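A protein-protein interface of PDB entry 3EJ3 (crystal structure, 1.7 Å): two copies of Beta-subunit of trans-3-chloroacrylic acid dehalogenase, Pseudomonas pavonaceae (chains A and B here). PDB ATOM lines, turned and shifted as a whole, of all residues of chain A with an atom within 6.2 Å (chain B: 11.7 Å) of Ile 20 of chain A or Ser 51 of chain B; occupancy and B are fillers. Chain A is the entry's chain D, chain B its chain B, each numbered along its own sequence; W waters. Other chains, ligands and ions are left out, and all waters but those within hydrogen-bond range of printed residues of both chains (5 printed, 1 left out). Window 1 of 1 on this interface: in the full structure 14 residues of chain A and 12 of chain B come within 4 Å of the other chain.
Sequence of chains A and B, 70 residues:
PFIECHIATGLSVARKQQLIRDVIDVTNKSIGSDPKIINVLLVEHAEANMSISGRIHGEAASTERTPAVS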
ATOM      1  N   ARG A  15      13.298   1.158 -17.572  1.00  0.00           N
ATOM      2  CA  ARG A  15      11.908   0.811 -17.336  1.00  0.00           C
ATOM      3  C   ARG A  15      11.353   1.571 -16.121  1.00  0.00           C
ATOM      4  O   ARG A  15      10.197   1.993 -16.125  1.00  0.00           O
ATOM      5  CB  ARG A  15      11.733  -0.694 -17.178  1.00  0.00           C
ATOM      6  CG  ARG A  15      10.264  -1.137 -17.095  1.00  0.00           C
ATOM      7  CD  ARG A  15       9.523  -0.815 -18.414  1.00  0.00           C
ATOM      8  NE  ARG A  15       8.079  -1.079 -18.383  1.00  0.00           N
ATOM      9  CZ  ARG A  15       7.172  -0.234 -17.897  1.00  0.00           C
ATOM     10  NH1 ARG A  15       5.886  -0.551 -17.939  1.00  0.00           N
ATOM     11  NH2 ARG A  15       7.551   0.936 -17.373  1.00  0.00           N
ATOM     12  N   LYS A  16      12.189   1.761 -15.104  1.00  0.00           N
ATOM     13  CA  LYS A  16      11.750   2.555 -13.933  1.00  0.00           C
ATOM     14  C   LYS A  16      11.477   4.008 -14.310  1.00  0.00           C
ATOM     15  O   LYS A  16      10.488   4.624 -13.859  1.00  0.00           O
ATOM     16  CB  LYS A  16      12.793   2.486 -12.829  1.00  0.00           C
ATOM     17  CG  LYS A  16      12.877   1.109 -12.203  1.00  0.00           C
ATOM     18  CD  LYS A  16      13.826   1.083 -11.002  1.00  0.00           C
ATOM     19  CE  LYS A  16      15.259   0.969 -11.456  1.00  0.00           C
ATOM     20  NZ  LYS A  16      16.131   0.245 -10.481  1.00  0.00           N
ATOM     21  N   GLN A  17      12.347   4.569 -15.146  1.00  0.00           N
ATOM     22  CA  GLN A  17      12.145   5.950 -15.605  1.00  0.00           C
ATOM     23  C   GLN A  17      10.875   6.125 -16.451  1.00  0.00           C
ATOM     24  O   GLN A  17      10.154   7.123 -16.291  1.00  0.00           O
ATOM     25  CB  GLN A  17      13.403   6.491 -16.289  1.00  0.00           C
ATOM     26  CG  GLN A  17      14.574   6.653 -15.299  1.00  0.00           C
ATOM     27  CD  GLN A  17      15.860   7.062 -15.955  1.00  0.00           C
ATOM     28  OE1 GLN A  17      16.507   8.026 -15.534  1.00  0.00           O
ATOM     29  NE2 GLN A  17      16.241   6.348 -16.991  1.00  0.00           N
ATOM     30  N   GLN A  18      10.580   5.128 -17.285  1.00  0.00           N
ATOM     31  CA  GLN A  18       9.328   5.064 -18.041  1.00  0.00           C
ATOM     32  C   GLN A  18       8.099   4.961 -17.107  1.00  0.00           C
ATOM     33  O   GLN A  18       7.092   5.630 -17.311  1.00  0.00           O
ATOM     34  CB  GLN A  18       9.352   3.880 -19.022  1.00  0.00           C
ATOM     35  CG  GLN A  18       8.061   3.748 -19.851  1.00  0.00           C
ATOM     36  CD  GLN A  18       7.839   4.911 -20.789  1.00  0.00           C
ATOM     37  OE1 GLN A  18       8.544   5.060 -21.791  1.00  0.00           O
ATOM     38  NE2 GLN A  18       6.845   5.749 -20.481  1.00  0.00           N
ATOM     39  N   LEU A  19       8.210   4.154 -16.062  1.00  0.00           N
ATOM     40  CA  LEU A  19       7.138   4.078 -15.058  1.00  0.00           C
ATOM     41  C   LEU A  19       6.900   5.453 -14.374  1.00  0.00           C
ATOM     42  O   LEU A  19       5.750   5.887 -14.223  1.00  0.00           O
ATOM     43  CB  LEU A  19       7.492   2.992 -14.019  1.00  0.00           C
ATOM     44  CG  LEU A  19       6.556   2.890 -12.801  1.00  0.00           C
ATOM     45  CD1 LEU A  19       5.111   2.597 -13.185  1.00  0.00           C
ATOM     46  CD2 LEU A  19       7.131   1.792 -11.888  1.00  0.00           C
ATOM     47  N   ILE A  20       7.972   6.135 -13.965  1.00  0.00           N
ATOM     48  CA  ILE A  20       7.866   7.481 -13.375  1.00  0.00           C
ATOM     49  C   ILE A  20       7.198   8.434 -14.361  1.00  0.00           C
ATOM     50  O   ILE A  20       6.289   9.166 -14.020  1.00  0.00           O
ATOM     51  CB  ILE A  20       9.251   8.019 -12.946  1.00  0.00           C
ATOM     52  CG1 ILE A  20       9.767   7.158 -11.781  1.00  0.00           C
ATOM     53  CG2 ILE A  20       9.185   9.508 -12.589  1.00  0.00           C
ATOM     54  CD1 ILE A  20      11.252   7.404 -11.419  1.00  0.00           C
ATOM     55  N   ARG A  21       7.622   8.359 -15.629  1.00  0.00           N
ATOM     56  CA  ARG A  21       6.971   9.161 -16.676  1.00  0.00           C
ATOM     57  C   ARG A  21       5.476   8.897 -16.772  1.00  0.00           C
ATOM     58  O   ARG A  21       4.684   9.852 -16.901  1.00  0.00           O
ATOM     59  CB  ARG A  21       7.643   8.900 -18.021  1.00  0.00           C
ATOM     60  CG  ARG A  21       7.162   9.860 -19.103  1.00  0.00           C
ATOM     61  CD  ARG A  21       8.015   9.725 -20.333  1.00  0.00           C
ATOM     62  NE  ARG A  21       9.446   9.866 -20.070  1.00  0.00           N
ATOM     63  CZ  ARG A  21      10.080  11.024 -19.958  1.00  0.00           C
ATOM     64  NH1 ARG A  21       9.408  12.171 -20.083  1.00  0.00           N
ATOM     65  NH2 ARG A  21      11.387  11.033 -19.749  1.00  0.00           N
ATOM     66  N   ASP A  22       5.079   7.621 -16.736  1.00  0.00           N
ATOM     67  CA  ASP A  22       3.654   7.255 -16.821  1.00  0.00           C
ATOM     68  C   ASP A  22       2.882   7.708 -15.593  1.00  0.00           C
ATOM     69  O   ASP A  22       1.737   8.111 -15.684  1.00  0.00           O
ATOM     70  CB  ASP A  22       3.490   5.756 -16.989  1.00  0.00           C
ATOM     71  CG  ASP A  22       4.007   5.260 -18.349  1.00  0.00           C
ATOM     72  OD1 ASP A  22       4.260   4.042 -18.486  1.00  0.00           O
ATOM     73  OD2 ASP A  22       4.169   6.095 -19.262  1.00  0.00           O
ATOM     74  N   VAL A  23       3.502   7.588 -14.422  1.00  0.00           N
ATOM     75  CA  VAL A  23       2.858   8.114 -13.205  1.00  0.00           C
ATOM     76  C   VAL A  23       2.595   9.614 -13.322  1.00  0.00           C
ATOM     77  O   VAL A  23       1.508  10.095 -12.968  1.00  0.00           O
ATOM     78  CB  VAL A  23       3.731   7.778 -11.983  1.00  0.00           C
ATOM     79  CG1 VAL A  23       3.332   8.635 -10.754  1.00  0.00           C
ATOM     80  CG2 VAL A  23       3.626   6.309 -11.680  1.00  0.00           C
ATOM     81  N   ILE A  24       3.595  10.375 -13.776  1.00  0.00           N
ATOM     82  CA  ILE A  24       3.398  11.815 -13.995  1.00  0.00           C
ATOM     83  C   ILE A  24       2.214  12.023 -14.948  1.00  0.00           C
ATOM     84  O   ILE A  24       1.282  12.831 -14.689  1.00  0.00           O
ATOM     85  CB  ILE A  24       4.694  12.484 -14.529  1.00  0.00           C
ATOM     86  CG1 ILE A  24       5.766  12.449 -13.432  1.00  0.00           C
ATOM     87  CG2 ILE A  24       4.422  13.936 -14.887  1.00  0.00           C
ATOM     88  CD1 ILE A  24       7.217  12.713 -13.922  1.00  0.00           C
ATOM     89  N   ASP A  25       2.236  11.281 -16.048  1.00  0.00           N
ATOM     90  CA  ASP A  25       1.222  11.450 -17.097  1.00  0.00           C
ATOM     91  C   ASP A  25      -0.183  11.161 -16.572  1.00  0.00           C
ATOM     92  O   ASP A  25      -1.089  11.968 -16.763  1.00  0.00           O
ATOM     93  CB  ASP A  25       1.524  10.534 -18.279  1.00  0.00           C
ATOM     94  CG  ASP A  25       0.550  10.718 -19.430  1.00  0.00           C
ATOM     95  OD1 ASP A  25      -0.023   9.696 -19.885  1.00  0.00           O
ATOM     96  OD2 ASP A  25       0.355  11.887 -19.873  1.00  0.00           O
ATOM     97  N   ILE A  38       4.384  17.781  -9.787  1.00  0.00           N
ATOM     98  CA  ILE A  38       4.255  16.355  -9.490  1.00  0.00           C
ATOM     99  C   ILE A  38       5.603  15.780  -9.078  1.00  0.00           C
ATOM    100  O   ILE A  38       6.603  15.942  -9.787  1.00  0.00           O
ATOM    101  CB  ILE A  38       3.683  15.572 -10.707  1.00  0.00           C
ATOM    102  CG1 ILE A  38       2.311  16.131 -11.083  1.00  0.00           C
ATOM    103  CG2 ILE A  38       3.599  14.075 -10.389  1.00  0.00           C
ATOM    104  CD1 ILE A  38       1.831  15.644 -12.391  1.00  0.00           C
ATOM    105  N   ASN A  39       5.648  15.100  -7.935  1.00  0.00           N
ATOM    106  CA  ASN A  39       6.899  14.532  -7.459  1.00  0.00           C
ATOM    107  C   ASN A  39       6.680  13.056  -7.297  1.00  0.00           C
ATOM    108  O   ASN A  39       5.620  12.634  -6.805  1.00  0.00           O
ATOM    109  CB  ASN A  39       7.272  15.171  -6.108  1.00  0.00           C
ATOM    110  CG  ASN A  39       7.328  16.697  -6.215  1.00  0.00           C
ATOM    111  OD1 ASN A  39       8.258  17.233  -6.833  1.00  0.00           O
ATOM    112  ND2 ASN A  39       6.309  17.386  -5.691  1.00  0.00           N
ATOM    113  N   VAL A  40       7.669  12.271  -7.697  1.00  0.00           N
ATOM    114  CA  VAL A  40       7.515  10.819  -7.691  1.00  0.00           C
ATOM    115  C   VAL A  40       8.723  10.172  -7.072  1.00  0.00           C
ATOM    116  O   VAL A  40       9.861  10.538  -7.379  1.00  0.00           O
ATOM    117  CB  VAL A  40       7.270  10.219  -9.153  1.00  0.00           C
ATOM    118  CG1 VAL A  40       6.938   8.740  -9.079  1.00  0.00           C
ATOM    119  CG2 VAL A  40       6.137  10.953  -9.891  1.00  0.00           C
ATOM    120  N   LEU A  41       8.471   9.174  -6.231  1.00  0.00           N
ATOM    121  CA  LEU A  41       9.542   8.357  -5.690  1.00  0.00           C
ATOM    122  C   LEU A  41       9.216   6.905  -5.907  1.00  0.00           C
ATOM    123  O   LEU A  41       8.145   6.421  -5.508  1.00  0.00           O
ATOM    124  CB  LEU A  41       9.681   8.606  -4.177  1.00  0.00           C
ATOM    125  CG  LEU A  41      10.744   7.835  -3.405  1.00  0.00           C
ATOM    126  CD1 LEU A  41      12.156   8.224  -3.903  1.00  0.00           C
ATOM    127  CD2 LEU A  41      10.563   8.169  -1.887  1.00  0.00           C
ATOM    128  N   LEU A  42      10.177   6.198  -6.504  1.00  0.00           N
ATOM    129  CA  LEU A  42      10.043   4.775  -6.694  1.00  0.00           C
ATOM    130  C   LEU A  42      10.957   4.055  -5.710  1.00  0.00           C
ATOM    131  O   LEU A  42      12.166   4.283  -5.689  1.00  0.00           O
ATOM    132  CB  LEU A  42      10.390   4.423  -8.141  1.00  0.00           C
ATOM    133  CG  LEU A  42      10.275   2.966  -8.520  1.00  0.00           C
ATOM    134  CD1 LEU A  42       8.837   2.499  -8.447  1.00  0.00           C
ATOM    135  CD2 LEU A  42      10.790   2.830  -9.954  1.00  0.00           C
ATOM    136  N   HIS B   6      14.119  11.878   2.143  1.00  0.00           N
ATOM    137  CA  HIS B   6      14.417  11.098   0.937  1.00  0.00           C
ATOM    138  C   HIS B   6      15.410  11.864   0.087  1.00  0.00           C
ATOM    139  O   HIS B   6      15.111  12.958  -0.407  1.00  0.00           O
ATOM    140  CB  HIS B   6      13.121  10.841   0.158  1.00  0.00           C
ATOM    141  CG  HIS B   6      12.211   9.888   0.864  1.00  0.00           C
ATOM    142  ND1 HIS B   6      11.085  10.285   1.562  1.00  0.00           N
ATOM    143  CD2 HIS B   6      12.332   8.563   1.070  1.00  0.00           C
ATOM    144  CE1 HIS B   6      10.525   9.221   2.119  1.00  0.00           C
ATOM    145  NE2 HIS B   6      11.257   8.167   1.830  1.00  0.00           N
ATOM    146  N   ILE B   7      16.618  11.327  -0.022  1.00  0.00           N
ATOM    147  CA  ILE B   7      17.679  12.009  -0.741  1.00  0.00           C
ATOM    148  C   ILE B   7      18.419  11.016  -1.665  1.00  0.00           C
ATOM    149  O   ILE B   7      18.248   9.801  -1.543  1.00  0.00           O
ATOM    150  CB  ILE B   7      18.722  12.640   0.244  1.00  0.00           C
ATOM    151  CG1 ILE B   7      19.455  11.558   1.027  1.00  0.00           C
ATOM    152  CG2 ILE B   7      18.053  13.624   1.221  1.00  0.00           C
ATOM    153  CD1 ILE B   7      20.689  12.144   1.749  1.00  0.00           C
ATOM    154  N   ALA B   8      19.220  11.576  -2.571  1.00  0.00           N
ATOM    155  CA  ALA B   8      20.041  10.782  -3.485  1.00  0.00           C
ATOM    156  C   ALA B   8      21.205  10.165  -2.714  1.00  0.00           C
ATOM    157  O   ALA B   8      21.702  10.760  -1.760  1.00  0.00           O
ATOM    158  CB  ALA B   8      20.571  11.649  -4.579  1.00  0.00           C
ATOM    159  N   HIS B  45      18.303   7.042  -2.147  1.00  0.00           N
ATOM    160  CA  HIS B  45      17.761   6.479  -3.375  1.00  0.00           C
ATOM    161  C   HIS B  45      18.653   6.796  -4.554  1.00  0.00           C
ATOM    162  O   HIS B  45      19.326   7.830  -4.595  1.00  0.00           O
ATOM    163  CB  HIS B  45      16.415   7.123  -3.681  1.00  0.00           C
ATOM    164  CG  HIS B  45      15.439   7.008  -2.573  1.00  0.00           C
ATOM    165  ND1 HIS B  45      14.688   5.876  -2.361  1.00  0.00           N
ATOM    166  CD2 HIS B  45      15.065   7.901  -1.628  1.00  0.00           C
ATOM    167  CE1 HIS B  45      13.899   6.071  -1.316  1.00  0.00           C
ATOM    168  NE2 HIS B  45      14.111   7.289  -0.856  1.00  0.00           N
ATOM    169  N   ALA B  46      18.634   5.902  -5.536  1.00  0.00           N
ATOM    170  CA  ALA B  46      19.238   6.236  -6.810  1.00  0.00           C
ATOM    171  C   ALA B  46      18.524   7.462  -7.395  1.00  0.00           C
ATOM    172  O   ALA B  46      17.293   7.574  -7.322  1.00  0.00           O
ATOM    173  CB  ALA B  46      19.145   5.067  -7.734  1.00  0.00           C
ATOM    174  N   GLU B  47      19.292   8.373  -7.974  1.00  0.00           N
ATOM    175  CA  GLU B  47      18.731   9.555  -8.658  1.00  0.00           C
ATOM    176  C   GLU B  47      17.638   9.172  -9.656  1.00  0.00           C
ATOM    177  O   GLU B  47      16.621   9.879  -9.753  1.00  0.00           O
ATOM    178  CB  GLU B  47      19.826  10.361  -9.383  1.00  0.00           C
ATOM    179  CG  GLU B  47      20.636  11.268  -8.482  1.00  0.00           C
ATOM    180  CD  GLU B  47      19.925  12.575  -8.101  1.00  0.00           C
ATOM    181  OE1 GLU B  47      20.639  13.482  -7.592  1.00  0.00           O
ATOM    182  OE2 GLU B  47      18.686  12.720  -8.313  1.00  0.00           O
ATOM    183  N   ALA B  48      17.831   8.051 -10.359  1.00  0.00           N
ATOM    184  CA  ALA B  48      16.877   7.583 -11.369  1.00  0.00           C
ATOM    185  C   ALA B  48      15.501   7.220 -10.781  1.00  0.00           C
ATOM    186  O   ALA B  48      14.490   7.226 -11.499  1.00  0.00           O
ATOM    187  CB  ALA B  48      17.435   6.389 -12.112  1.00  0.00           C
ATOM    188  N   ASN B  49      15.481   6.896  -9.481  1.00  0.00           N
ATOM    189  CA  ASN B  49      14.256   6.527  -8.797  1.00  0.00           C
ATOM    190  C   ASN B  49      13.433   7.718  -8.273  1.00  0.00           C
ATOM    191  O   ASN B  49      12.371   7.516  -7.674  1.00  0.00           O
ATOM    192  CB  ASN B  49      14.597   5.582  -7.632  1.00  0.00           C
ATOM    193  CG  ASN B  49      14.895   4.173  -8.089  1.00  0.00           C
ATOM    194  OD1 ASN B  49      15.667   3.956  -9.020  1.00  0.00           O
ATOM    195  ND2 ASN B  49      14.302   3.194  -7.410  1.00  0.00           N
ATOM    196  N   MET B  50      13.915   8.939  -8.513  1.00  0.00           N
ATOM    197  CA  MET B  50      13.305  10.174  -7.987  1.00  0.00           C
ATOM    198  C   MET B  50      12.988  11.164  -9.106  1.00  0.00           C
ATOM    199  O   MET B  50      13.849  11.410  -9.981  1.00  0.00           O
ATOM    200  CB  MET B  50      14.236  10.858  -6.971  1.00  0.00           C
ATOM    201  CG  MET B  50      14.809   9.915  -5.932  1.00  0.00           C
ATOM    202  SD  MET B  50      15.661  10.862  -4.638  1.00  0.00           S
ATOM    203  CE  MET B  50      17.223  10.901  -5.371  1.00  0.00           C
ATOM    204  N   SER B  51      11.775  11.732  -9.083  1.00  0.00           N
ATOM    205  CA  SER B  51      11.425  12.850  -9.962  1.00  0.00           C
ATOM    206  C   SER B  51      10.897  14.018  -9.133  1.00  0.00           C
ATOM    207  O   SER B  51       9.923  13.847  -8.385  1.00  0.00           O
ATOM    208  CB  SER B  51      10.377  12.448 -11.003  1.00  0.00           C
ATOM    209  OG  SER B  51      10.010  13.600 -11.740  1.00  0.00           O
ATOM    210  N   ILE B  52      11.575  15.167  -9.231  1.00  0.00           N
ATOM    211  CA  ILE B  52      11.150  16.409  -8.580  1.00  0.00           C
ATOM    212  C   ILE B  52      10.583  17.309  -9.676  1.00  0.00           C
ATOM    213  O   ILE B  52      11.206  17.442 -10.732  1.00  0.00           O
ATOM    214  CB  ILE B  52      12.348  17.109  -7.866  1.00  0.00           C
ATOM    215  CG1 ILE B  52      12.769  16.307  -6.627  1.00  0.00           C
ATOM    216  CG2 ILE B  52      11.981  18.537  -7.442  1.00  0.00           C
ATOM    217  CD1 ILE B  52      11.681  16.191  -5.548  1.00  0.00           C
ATOM    218  N   SER B  53       9.402  17.886  -9.449  1.00  0.00           N
ATOM    219  CA  SER B  53       8.782  18.778 -10.430  1.00  0.00           C
ATOM    220  C   SER B  53       8.702  18.147 -11.835  1.00  0.00           C
ATOM    221  O   SER B  53       8.937  18.839 -12.837  1.00  0.00           O
ATOM    222  CB  SER B  53       9.556  20.105 -10.521  1.00  0.00           C
ATOM    223  OG  SER B  53       9.688  20.718  -9.244  1.00  0.00           O
ATOM    224  N   GLY B  54       8.399  16.855 -11.889  1.00  0.00           N
ATOM    225  CA  GLY B  54       8.130  16.161 -13.147  1.00  0.00           C
ATOM    226  C   GLY B  54       9.349  15.881 -14.016  1.00  0.00           C
ATOM    227  O   GLY B  54       9.198  15.446 -15.172  1.00  0.00           O
ATOM    228  N   ARG B  55      10.544  16.096 -13.468  1.00  0.00           N
ATOM    229  CA  ARG B  55      11.790  15.972 -14.237  1.00  0.00           C
ATOM    230  C   ARG B  55      12.339  14.577 -14.247  1.00  0.00           C
ATOM    231  O   ARG B  55      12.374  13.894 -13.218  1.00  0.00           O
ATOM    232  CB  ARG B  55      12.858  16.950 -13.726  1.00  0.00           C
ATOM    233  CG  ARG B  55      12.366  18.398 -13.819  1.00  0.00           C
ATOM    234  CD  ARG B  55      13.482  19.392 -13.617  1.00  0.00           C
ATOM    235  NE  ARG B  55      13.973  19.389 -12.249  1.00  0.00           N
ATOM    236  CZ  ARG B  55      13.603  20.265 -11.312  1.00  0.00           C
ATOM    237  NH1 ARG B  55      14.111  20.185 -10.093  1.00  0.00           N
ATOM    238  NH2 ARG B  55      12.729  21.225 -11.583  1.00  0.00           N
ATOM    239  N   ILE B  56      12.772  14.165 -15.439  1.00  0.00           N
ATOM    240  CA  ILE B  56      13.400  12.874 -15.661  1.00  0.00           C
ATOM    241  C   ILE B  56      14.565  13.199 -16.596  1.00  0.00           C
ATOM    242  O   ILE B  56      14.391  13.981 -17.541  1.00  0.00           O
ATOM    243  CB  ILE B  56      12.425  11.851 -16.322  1.00  0.00           C
ATOM    244  CG1 ILE B  56      11.167  11.650 -15.455  1.00  0.00           C
ATOM    245  CG2 ILE B  56      13.102  10.533 -16.485  1.00  0.00           C
ATOM    246  CD1 ILE B  56      10.065  10.853 -16.083  1.00  0.00           C
ATOM    247  N   HIS B  57      15.749  12.650 -16.310  1.00  0.00           N
ATOM    248  CA  HIS B  57      16.984  13.035 -17.036  1.00  0.00           C
ATOM    249  C   HIS B  57      17.224  14.549 -16.983  1.00  0.00           C
ATOM    250  O   HIS B  57      17.826  15.141 -17.885  1.00  0.00           O
ATOM    251  CB  HIS B  57      16.948  12.588 -18.511  1.00  0.00           C
ATOM    252  CG  HIS B  57      16.405  11.213 -18.733  1.00  0.00           C
ATOM    253  ND1 HIS B  57      17.072  10.078 -18.334  1.00  0.00           N
ATOM    254  CD2 HIS B  57      15.279  10.786 -19.357  1.00  0.00           C
ATOM    255  CE1 HIS B  57      16.374   9.011 -18.675  1.00  0.00           C
ATOM    256  NE2 HIS B  57      15.284   9.411 -19.304  1.00  0.00           N
ATOM    257  N   GLY B  58      16.732  15.179 -15.918  1.00  0.00           N
ATOM    258  CA  GLY B  58      16.906  16.607 -15.715  1.00  0.00           C
ATOM    259  C   GLY B  58      15.917  17.460 -16.482  1.00  0.00           C
ATOM    260  O   GLY B  58      15.971  18.684 -16.397  1.00  0.00           O
ATOM    261  N   GLU B  59      15.002  16.819 -17.218  1.00  0.00           N
ATOM    262  CA  GLU B  59      14.054  17.539 -18.087  1.00  0.00           C
ATOM    263  C   GLU B  59      12.589  17.258 -17.766  1.00  0.00           C
ATOM    264  O   GLU B  59      12.193  16.094 -17.622  1.00  0.00           O
ATOM    265  CB  GLU B  59      14.358  17.248 -19.565  1.00  0.00           C
ATOM    266  CG  GLU B  59      15.772  17.702 -20.006  1.00  0.00           C
ATOM    267  CD  GLU B  59      16.088  19.179 -19.665  1.00  0.00           C
ATOM    268  OE1 GLU B  59      15.138  19.996 -19.530  1.00  0.00           O
ATOM    269  OE2 GLU B  59      17.289  19.529 -19.532  1.00  0.00           O
ATOM    270  N   ALA B  60      11.787  18.328 -17.680  1.00  0.00           N
ATOM    271  CA  ALA B  60      10.382  18.194 -17.276  1.00  0.00           C
ATOM    272  C   ALA B  60       9.557  17.386 -18.277  1.00  0.00           C
ATOM    273  O   ALA B  60       9.856  17.366 -19.480  1.00  0.00           O
ATOM    274  CB  ALA B  60       9.750  19.558 -17.020  1.00  0.00           C
ATOM    275  N   ALA B  61       8.526  16.714 -17.763  1.00  0.00           N
ATOM    276  CA  ALA B  61       7.708  15.806 -18.561  1.00  0.00           C
ATOM    277  C   ALA B  61       6.631  16.550 -19.357  1.00  0.00           C
ATOM    278  O   ALA B  61       6.684  17.778 -19.497  1.00  0.00           O
ATOM    279  CB  ALA B  61       7.087  14.726 -17.673  1.00  0.00           C
HETATM  280  O   HOH W   1      10.850  14.799 -19.673  1.00  0.00           O
HETATM  281  O   HOH W   2      13.142  13.553 -19.772  1.00  0.00           O
HETATM  282  O   HOH W   3      19.032   9.867 -16.436  1.00  0.00           O
HETATM  283  O   HOH W   4      15.990  11.013 -13.950  1.00  0.00           O
HETATM  284  O   HOH W   5      14.510   4.040  -4.328  1.00  0.00           O
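The backbone carbonyl oxygen (O) of Arg 55 of chain B is in hydrogen-bond range of the side-chain hydroxyl (OG) of Ser 51 of chain B, at 2.8 Å. The backbone carbonyl oxygen (O) of Gly 54 of chain B lies within hydrogen-bond range of the backbone NH (N) of Ala 61 of chain B, 3.0 Å away. The backbone carbonyl oxygen (O) of Ile 7 of chain B lies within hydrogen-bond range of the backbone NH (N) of His 45 of chain B, at 2.8 Å.
O of Ile 38 of chain A is in hydrogen-bond range of N of Ser 53 of chain B, 3.4 Å away. O of Asn 49 of chain B is in hydrogen-bond range of N of Leu 42 of chain A. The backbone carbonyl oxygen of Ile 38 of chain A is in hydrogen-bond range of the backbone NH of Gly 54 of chain B (2.9 Å). The backbone NH of Ser 51 of chain B lies within hydrogen-bond range of the backbone carbonyl oxygen of Val 40 of chain A (2.8 Å). The backbone NH of Ser 53 of chain B is in hydrogen-bond range of the side-chain amide oxygen of Asn 39 of chain A (2.9 Å).
No position is printed for both chains. Of the 26 pairs that touch across the chains among the printed residues, none has its exchanged pair printed and touching as well.
CE of Lys 16 of chain A touches OD1 of Asn 49 of chain B, 3.9 Å away. Arg 21 of chain A touches Ile 56 of chain B. Arg 21 of chain A touches His 57 of chain B (NH2 to CD2, 3.9 Å). CD1 of Ile 24 of chain A touches O of Gly 54 of chain B (3.6 Å). Asn 39 of chain A touches Ser 51 of chain B (CA to O, 3.2 Å). CA of Ile 52 of chain B touches OD1 of Asn 39 of chain A, at 3.5 Å. Met 50 of chain B touches Val 40 of chain A (CA to O, 3.5 Å). His 6 of chain B touches Leu 41 of chain A. Leu 41 of chain A touches His 45 of chain B (CD1 to CD2, 3.7 Å). Leu 41 of chain A touches Asn 49 of chain B.
Of chain B, only Ala 48, Asn 49, Ser 51 and Ile 56 come within 4 Å of Ile 20 of chain A. Ser 51 of chain B touches just these residues of chain A: Ile 20, Ile 24, Asn 39 and Val 40. Gln 17 of chain A touches just these residues of chain B: Ala 48 (3.8 Å), Ile 56 (3.7 Å) and His 57 (3.2 Å). No residue of chain B comes within 4 Å of Leu 19 of chain A. Arg 21 of chain A touches just these residues of chain B: Ile 56 and His 57. No residue of chain B comes within 4 Å of Asp 22 of chain A. Of chain B, only Ser 51 (3.7 Å), Gly 54 (3.6 Å) and Ala 61 (3.9 Å) come within 4 Å of Ile 24 of chain A. Of chain B, only Asn 49 (3.9 Å), Met 50 (3.5 Å) and Ser 51 (2.8 Å) come within 4 Å of Val 40 of chain A. Printed residues of chain B within 4 Å of Lys 16 of chain A: Asn 49. Printed residues of chain A within 4 Å of His 45 of chain B: Leu 41. Printed residues of chain A within 4 Å of Ile 56 of chain B: Gln 17, Ile 20 and Arg 21. Of the printed residues of chain A, Ala 61 of chain B touches Ile 24. Printed residues of chain A within 4 Å of Ala 48 of chain B: Gln 17 (3.8 Å) and Ile 20 (3.2 Å). Ala 60 of chain B touches none of the printed residues of chain A. Ile 7 of chain B touches none of the printed residues of chain A. The nearest printed residue of chain A that does not touch His 6 of chain B is Leu 42 of chain A (8.0 Å).
Water W2 lies within hydrogen-bond range of the backbone carbonyl oxygen (O) of Ile 56 of chain B, the guanidinium group (NH2) of Arg 21 of chain A and the backbone carbonyl oxygen (O) of Glu 59 of chain B. Water W5 lies within hydrogen-bond range of ND1 of His 45 of chain B (2.7 Å), O of Leu 42 of chain A (2.7 Å) and ND2 of Asn 49 of chain B (3.2 Å). Water W3 bridges a ring nitrogen (ND1) of His 57 of chain B (2.7 Å) and the side-chain amide oxygen of Gln 17 of chain A (3.3 Å). Water W1 lies within hydrogen-bond range of O of Ala 60 of chain B, O of Glu 59 of chain B and NH1 of Arg 21 of chain A. Water W4 lies within hydrogen-bond range of N of His 57 of chain B (2.9 Å) and OE1 of Gln 17 of chain A (3.4 Å).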
